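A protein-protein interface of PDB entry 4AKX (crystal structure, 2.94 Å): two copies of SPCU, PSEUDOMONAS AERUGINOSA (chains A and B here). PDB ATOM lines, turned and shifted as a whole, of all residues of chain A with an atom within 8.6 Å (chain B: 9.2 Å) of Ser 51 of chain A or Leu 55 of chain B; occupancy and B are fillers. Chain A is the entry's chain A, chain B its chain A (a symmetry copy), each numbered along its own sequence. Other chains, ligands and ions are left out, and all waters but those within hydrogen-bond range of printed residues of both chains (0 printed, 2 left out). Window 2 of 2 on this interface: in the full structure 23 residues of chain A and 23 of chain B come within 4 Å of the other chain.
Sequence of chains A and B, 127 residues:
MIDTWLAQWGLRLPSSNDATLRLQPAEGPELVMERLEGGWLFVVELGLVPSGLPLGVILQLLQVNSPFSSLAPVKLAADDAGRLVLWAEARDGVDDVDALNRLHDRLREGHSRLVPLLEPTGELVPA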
ATOM      1  N   LEU A  48      -5.118  -4.193  18.894  1.00  0.00           N
ATOM      2  CA  LEU A  48      -5.915  -4.204  20.120  1.00  0.00           C
ATOM      3  C   LEU A  48      -6.031  -2.800  20.667  1.00  0.00           C
ATOM      4  O   LEU A  48      -5.048  -2.053  20.693  1.00  0.00           O
ATOM      5  CB  LEU A  48      -5.271  -5.112  21.188  1.00  0.00           C
ATOM      6  CG  LEU A  48      -5.198  -6.607  20.867  1.00  0.00           C
ATOM      7  CD1 LEU A  48      -4.579  -7.418  21.983  1.00  0.00           C
ATOM      8  CD2 LEU A  48      -6.572  -7.161  20.526  1.00  0.00           C
ATOM      9  N   VAL A  49      -7.228  -2.450  21.125  1.00  0.00           N
ATOM     10  CA  VAL A  49      -7.437  -1.178  21.767  1.00  0.00           C
ATOM     11  C   VAL A  49      -6.421  -0.974  22.884  1.00  0.00           C
ATOM     12  O   VAL A  49      -6.167  -1.873  23.701  1.00  0.00           O
ATOM     13  CB  VAL A  49      -8.855  -1.046  22.311  1.00  0.00           C
ATOM     14  CG1 VAL A  49      -9.021   0.291  23.002  1.00  0.00           C
ATOM     15  CG2 VAL A  49      -9.864  -1.131  21.196  1.00  0.00           C
ATOM     16  N   PRO A  50      -5.779   0.196  22.891  1.00  0.00           N
ATOM     17  CA  PRO A  50      -4.769   0.466  23.905  1.00  0.00           C
ATOM     18  C   PRO A  50      -5.425   0.882  25.186  1.00  0.00           C
ATOM     19  O   PRO A  50      -6.552   1.389  25.174  1.00  0.00           O
ATOM     20  CB  PRO A  50      -3.998   1.657  23.336  1.00  0.00           C
ATOM     21  CG  PRO A  50      -4.402   1.762  21.910  1.00  0.00           C
ATOM     22  CD  PRO A  50      -5.775   1.198  21.819  1.00  0.00           C
ATOM     23  N   SER A  51      -4.715   0.634  26.283  1.00  0.00           N
ATOM     24  CA  SER A  51      -5.052   1.117  27.610  1.00  0.00           C
ATOM     25  C   SER A  51      -4.653   2.580  27.691  1.00  0.00           C
ATOM     26  O   SER A  51      -3.748   3.019  26.982  1.00  0.00           O
ATOM     27  CB  SER A  51      -4.256   0.295  28.634  1.00  0.00           C
ATOM     28  OG  SER A  51      -4.325   0.850  29.939  1.00  0.00           O
ATOM     29  N   GLY A  52      -5.324   3.335  28.549  1.00  0.00           N
ATOM     30  CA  GLY A  52      -4.982   4.743  28.775  1.00  0.00           C
ATOM     31  C   GLY A  52      -5.045   5.700  27.586  1.00  0.00           C
ATOM     32  O   GLY A  52      -4.207   6.567  27.453  1.00  0.00           O
ATOM     33  N   LEU A  53      -6.036   5.563  26.721  1.00  0.00           N
ATOM     34  CA  LEU A  53      -6.213   6.553  25.670  1.00  0.00           C
ATOM     35  C   LEU A  53      -6.704   7.870  26.279  1.00  0.00           C
ATOM     36  O   LEU A  53      -7.467   7.850  27.231  1.00  0.00           O
ATOM     37  CB  LEU A  53      -7.216   6.053  24.625  1.00  0.00           C
ATOM     38  CG  LEU A  53      -6.738   5.114  23.498  1.00  0.00           C
ATOM     39  CD1 LEU A  53      -7.775   5.085  22.388  1.00  0.00           C
ATOM     40  CD2 LEU A  53      -5.393   5.522  22.938  1.00  0.00           C
ATOM     41  N   PRO A  54      -6.240   9.015  25.755  1.00  0.00           N
ATOM     42  CA  PRO A  54      -6.831  10.284  26.177  1.00  0.00           C
ATOM     43  C   PRO A  54      -8.199  10.471  25.592  1.00  0.00           C
ATOM     44  O   PRO A  54      -8.525   9.882  24.565  1.00  0.00           O
ATOM     45  CB  PRO A  54      -5.891  11.334  25.596  1.00  0.00           C
ATOM     46  CG  PRO A  54      -5.062  10.618  24.586  1.00  0.00           C
ATOM     47  CD  PRO A  54      -4.967   9.211  25.056  1.00  0.00           C
ATOM     48  N   ILE A  58     -10.257   9.076  22.102  1.00  0.00           N
ATOM     49  CA  ILE A  58     -11.526   8.352  22.172  1.00  0.00           C
ATOM     50  C   ILE A  58     -12.536   9.030  21.266  1.00  0.00           C
ATOM     51  O   ILE A  58     -13.285   8.356  20.555  1.00  0.00           O
ATOM     52  CB  ILE A  58     -12.150   8.381  23.556  1.00  0.00           C
ATOM     53  CG1 ILE A  58     -11.310   7.641  24.583  1.00  0.00           C
ATOM     54  CG2 ILE A  58     -13.513   7.765  23.478  1.00  0.00           C
ATOM     55  CD1 ILE A  58     -10.784   6.307  24.087  1.00  0.00           C
ATOM     56  N   GLY A  82     -11.367  -7.570  21.369  1.00  0.00           N
ATOM     57  CA  GLY A  82     -10.936  -6.234  21.737  1.00  0.00           C
ATOM     58  C   GLY A  82     -10.063  -5.606  20.674  1.00  0.00           C
ATOM     59  O   GLY A  82      -9.339  -4.653  20.936  1.00  0.00           O
ATOM     60  N   LEU A 117      -2.525   7.295  15.909  1.00  0.00           N
ATOM     61  CA  LEU A 117      -3.129   7.635  17.191  1.00  0.00           C
ATOM     62  C   LEU A 117      -2.983   6.563  18.285  1.00  0.00           C
ATOM     63  O   LEU A 117      -3.102   6.860  19.476  1.00  0.00           O
ATOM     64  CB  LEU A 117      -4.604   7.904  17.016  1.00  0.00           C
ATOM     65  CG  LEU A 117      -5.067   8.854  15.930  1.00  0.00           C
ATOM     66  CD1 LEU A 117      -6.594   8.787  15.860  1.00  0.00           C
ATOM     67  CD2 LEU A 117      -4.588  10.264  16.225  1.00  0.00           C
ATOM     68  N   LEU A 118      -2.790   5.313  17.891  1.00  0.00           N
ATOM     69  CA  LEU A 118      -2.716   4.223  18.861  1.00  0.00           C
ATOM     70  C   LEU A 118      -1.280   3.910  19.254  1.00  0.00           C
ATOM     71  O   LEU A 118      -0.928   3.939  20.426  1.00  0.00           O
ATOM     72  CB  LEU A 118      -3.364   2.967  18.292  1.00  0.00           C
ATOM     73  CG  LEU A 118      -4.847   2.957  17.897  1.00  0.00           C
ATOM     74  CD1 LEU A 118      -5.249   4.140  17.041  1.00  0.00           C
ATOM     75  CD2 LEU A 118      -5.142   1.675  17.152  1.00  0.00           C
ATOM     76  N   PRO A 120       1.722   5.523  19.213  1.00  0.00           N
ATOM     77  CA  PRO A 120       2.286   6.504  20.153  1.00  0.00           C
ATOM     78  C   PRO A 120       1.629   6.529  21.533  1.00  0.00           C
ATOM     79  O   PRO A 120       2.023   7.329  22.389  1.00  0.00           O
ATOM     80  CB  PRO A 120       2.059   7.837  19.434  1.00  0.00           C
ATOM     81  CG  PRO A 120       2.212   7.477  18.001  1.00  0.00           C
ATOM     82  CD  PRO A 120       1.563   6.113  17.867  1.00  0.00           C
ATOM     83  N   THR A 121       0.637   5.669  21.743  1.00  0.00           N
ATOM     84  CA  THR A 121       0.103   5.459  23.080  1.00  0.00           C
ATOM     85  C   THR A 121       0.623   4.139  23.656  1.00  0.00           C
ATOM     86  O   THR A 121       1.849   3.917  23.720  1.00  0.00           O
ATOM     87  CB  THR A 121      -1.443   5.484  23.096  1.00  0.00           C
ATOM     88  OG1 THR A 121      -1.917   6.630  22.370  1.00  0.00           O
ATOM     89  CG2 THR A 121      -1.968   5.548  24.535  1.00  0.00           C
ATOM     90  N   GLY B  52     -11.891  10.037  31.597  1.00  0.00           N
ATOM     91  CA  GLY B  52     -11.460   8.907  32.425  1.00  0.00           C
ATOM     92  C   GLY B  52     -12.295   7.627  32.390  1.00  0.00           C
ATOM     93  O   GLY B  52     -12.485   6.992  33.406  1.00  0.00           O
ATOM     94  N   LEU B  53     -12.788   7.231  31.228  1.00  0.00           N
ATOM     95  CA  LEU B  53     -13.451   5.939  31.134  1.00  0.00           C
ATOM     96  C   LEU B  53     -12.416   4.818  31.267  1.00  0.00           C
ATOM     97  O   LEU B  53     -11.299   4.965  30.797  1.00  0.00           O
ATOM     98  CB  LEU B  53     -14.191   5.813  29.798  1.00  0.00           C
ATOM     99  CG  LEU B  53     -15.604   6.417  29.651  1.00  0.00           C
ATOM    100  CD1 LEU B  53     -16.279   5.831  28.423  1.00  0.00           C
ATOM    101  CD2 LEU B  53     -16.463   6.184  30.875  1.00  0.00           C
ATOM    102  N   PRO B  54     -12.773   3.711  31.937  1.00  0.00           N
ATOM    103  CA  PRO B  54     -11.887   2.548  31.917  1.00  0.00           C
ATOM    104  C   PRO B  54     -11.923   1.857  30.587  1.00  0.00           C
ATOM    105  O   PRO B  54     -12.893   1.981  29.844  1.00  0.00           O
ATOM    106  CB  PRO B  54     -12.477   1.624  32.976  1.00  0.00           C
ATOM    107  CG  PRO B  54     -13.846   2.146  33.250  1.00  0.00           C
ATOM    108  CD  PRO B  54     -13.785   3.608  32.991  1.00  0.00           C
ATOM    109  N   LEU B  55     -10.861   1.125  30.290  1.00  0.00           N
ATOM    110  CA  LEU B  55     -10.725   0.414  29.018  1.00  0.00           C
ATOM    111  C   LEU B  55     -11.969  -0.408  28.688  1.00  0.00           C
ATOM    112  O   LEU B  55     -12.567  -0.195  27.639  1.00  0.00           O
ATOM    113  CB  LEU B  55      -9.512  -0.492  29.067  1.00  0.00           C
ATOM    114  CG  LEU B  55      -9.117  -1.133  27.769  1.00  0.00           C
ATOM    115  CD1 LEU B  55      -9.149  -0.106  26.645  1.00  0.00           C
ATOM    116  CD2 LEU B  55      -7.734  -1.739  27.900  1.00  0.00           C
ATOM    117  N   GLY B  56     -12.349  -1.330  29.594  1.00  0.00           N
ATOM    118  CA  GLY B  56     -13.499  -2.245  29.421  1.00  0.00           C
ATOM    119  C   GLY B  56     -14.764  -1.554  28.963  1.00  0.00           C
ATOM    120  O   GLY B  56     -15.477  -2.045  28.072  1.00  0.00           O
ATOM    121  N   VAL B  57     -15.016  -0.373  29.521  1.00  0.00           N
ATOM    122  CA  VAL B  57     -16.143   0.450  29.093  1.00  0.00           C
ATOM    123  C   VAL B  57     -15.930   0.930  27.678  1.00  0.00           C
ATOM    124  O   VAL B  57     -16.808   0.761  26.832  1.00  0.00           O
ATOM    125  CB  VAL B  57     -16.336   1.659  30.016  1.00  0.00           C
ATOM    126  CG1 VAL B  57     -17.517   2.500  29.572  1.00  0.00           C
ATOM    127  CG2 VAL B  57     -16.505   1.198  31.460  1.00  0.00           C
ATOM    128  N   ILE B  58     -14.759   1.494  27.396  1.00  0.00           N
ATOM    129  CA  ILE B  58     -14.449   1.874  26.017  1.00  0.00           C
ATOM    130  C   ILE B  58     -14.778   0.715  25.096  1.00  0.00           C
ATOM    131  O   ILE B  58     -15.340   0.919  24.017  1.00  0.00           O
ATOM    132  CB  ILE B  58     -12.973   2.151  25.797  1.00  0.00           C
ATOM    133  CG1 ILE B  58     -12.491   3.366  26.574  1.00  0.00           C
ATOM    134  CG2 ILE B  58     -12.739   2.361  24.333  1.00  0.00           C
ATOM    135  CD1 ILE B  58     -13.439   4.549  26.494  1.00  0.00           C
ATOM    136  N   LEU B  59     -14.418  -0.504  25.529  1.00  0.00           N
ATOM    137  CA  LEU B  59     -14.500  -1.688  24.688  1.00  0.00           C
ATOM    138  C   LEU B  59     -15.936  -2.015  24.406  1.00  0.00           C
ATOM    139  O   LEU B  59     -16.346  -2.182  23.236  1.00  0.00           O
ATOM    140  CB  LEU B  59     -13.834  -2.864  25.362  1.00  0.00           C
ATOM    141  CG  LEU B  59     -12.362  -3.021  25.012  1.00  0.00           C
ATOM    142  CD1 LEU B  59     -11.637  -3.890  26.030  1.00  0.00           C
ATOM    143  CD2 LEU B  59     -12.251  -3.646  23.638  1.00  0.00           C
ATOM    144  N   GLN B  60     -16.717  -2.061  25.478  1.00  0.00           N
ATOM    145  CA  GLN B  60     -18.140  -2.313  25.359  1.00  0.00           C
ATOM    146  C   GLN B  60     -18.795  -1.264  24.450  1.00  0.00           C
ATOM    147  O   GLN B  60     -19.686  -1.591  23.697  1.00  0.00           O
ATOM    148  CB  GLN B  60     -18.775  -2.360  26.745  1.00  0.00           C
ATOM    149  CG  GLN B  60     -20.285  -2.387  26.764  1.00  0.00           C
ATOM    150  CD  GLN B  60     -20.809  -3.011  28.036  1.00  0.00           C
ATOM    151  OE1 GLN B  60     -20.086  -3.133  29.019  1.00  0.00           O
ATOM    152  NE2 GLN B  60     -22.065  -3.430  28.019  1.00  0.00           N
ATOM    153  N   LEU B  61     -18.293  -0.032  24.463  1.00  0.00           N
ATOM    154  CA  LEU B  61     -18.757   0.958  23.505  1.00  0.00           C
ATOM    155  C   LEU B  61     -18.440   0.597  22.053  1.00  0.00           C
ATOM    156  O   LEU B  61     -19.330   0.378  21.248  1.00  0.00           O
ATOM    157  CB  LEU B  61     -18.225   2.331  23.842  1.00  0.00           C
ATOM    158  CG  LEU B  61     -18.705   2.931  25.169  1.00  0.00           C
ATOM    159  CD1 LEU B  61     -18.366   4.407  25.229  1.00  0.00           C
ATOM    160  CD2 LEU B  61     -20.199   2.744  25.307  1.00  0.00           C
ATOM    161  N   LEU B  62     -17.173   0.463  21.737  1.00  0.00           N
ATOM    162  CA  LEU B  62     -16.781   0.000  20.418  1.00  0.00           C
ATOM    163  C   LEU B  62     -17.480  -1.281  19.970  1.00  0.00           C
ATOM    164  O   LEU B  62     -17.854  -1.420  18.796  1.00  0.00           O
ATOM    165  CB  LEU B  62     -15.273  -0.157  20.384  1.00  0.00           C
ATOM    166  CG  LEU B  62     -14.626   1.194  20.750  1.00  0.00           C
ATOM    167  CD1 LEU B  62     -13.135   1.084  20.986  1.00  0.00           C
ATOM    168  CD2 LEU B  62     -14.894   2.247  19.686  1.00  0.00           C
ATOM    169  N   GLN B  63     -17.690  -2.211  20.899  1.00  0.00           N
ATOM    170  CA  GLN B  63     -18.294  -3.477  20.514  1.00  0.00           C
ATOM    171  C   GLN B  63     -19.742  -3.353  20.019  1.00  0.00           C
ATOM    172  O   GLN B  63     -20.177  -4.161  19.208  1.00  0.00           O
ATOM    173  CB  GLN B  63     -18.160  -4.511  21.621  1.00  0.00           C
ATOM    174  CG  GLN B  63     -16.720  -4.972  21.834  1.00  0.00           C
ATOM    175  CD  GLN B  63     -16.572  -5.946  22.985  1.00  0.00           C
ATOM    176  OE1 GLN B  63     -17.337  -5.909  23.943  1.00  0.00           O
ATOM    177  NE2 GLN B  63     -15.582  -6.830  22.890  1.00  0.00           N
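Ile 58 of chain A touches its own counterpart, Ile 58 of chain B. Of the 6 pairs that touch across the chains among the printed residues, 1 has its exchanged pair printed and touching as well.
Pro 50 of chain A touches just one residue of chain B: Leu 55. Of chain B, only Leu 55 (3.9 Å) comes within 4 Å of Ser 51 of chain A. No residue of chain B comes within 4 Å of Gly 52 of chain A. Of chain A, only Val 49 (3.7 Å), Pro 50 (3.3 Å) and Ser 51 (3.9 Å) come within 4 Å of Leu 55 of chain B. Printed residues of chain A within 4 Å of Leu 59 of chain B: Gly 82 (3.5 Å). Printed residues of chain A within 4 Å of Leu 62 of chain B: Val 49. Gln 63 of chain B touches none of the printed residues of chain A.
Among the printed residues, pairs that only touch across the chains: Pro 50 of chain A with Leu 55 of chain B (3.3 Å), Gly 82 of chain A with Leu 59 of chain B (3.5 Å), Val 49 of chain A with Leu 55 of chain B (3.7 Å), Ser 51 of chain A with Leu 55 of chain B (3.9 Å), Val 49 of chain A with Leu 62 of chain B (3.96 Å) and Ile 58 of chain A with Ile 58 of chain B (3.99 Å).
Hydrophobic or aromatic side chains of chain A within 4 Å of the printed part of chain B: Val 49 and Ile 58. Of the 12 printed residues of chain B, 4 touch a printed residue of chain A. Hydrophobic or aromatic side chains of chain B that line the printed part of chain A: Leu 55, Ile 58, Leu 59 and Leu 62. Among the printed residues, no Asp or Glu carboxylate lies within 4 Å of a Lys or Arg side-chain nitrogen of the other chain.
N of Val 49 of chain A is in hydrogen-bond range of O of Gly 82 of chain A (3.1 Å).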
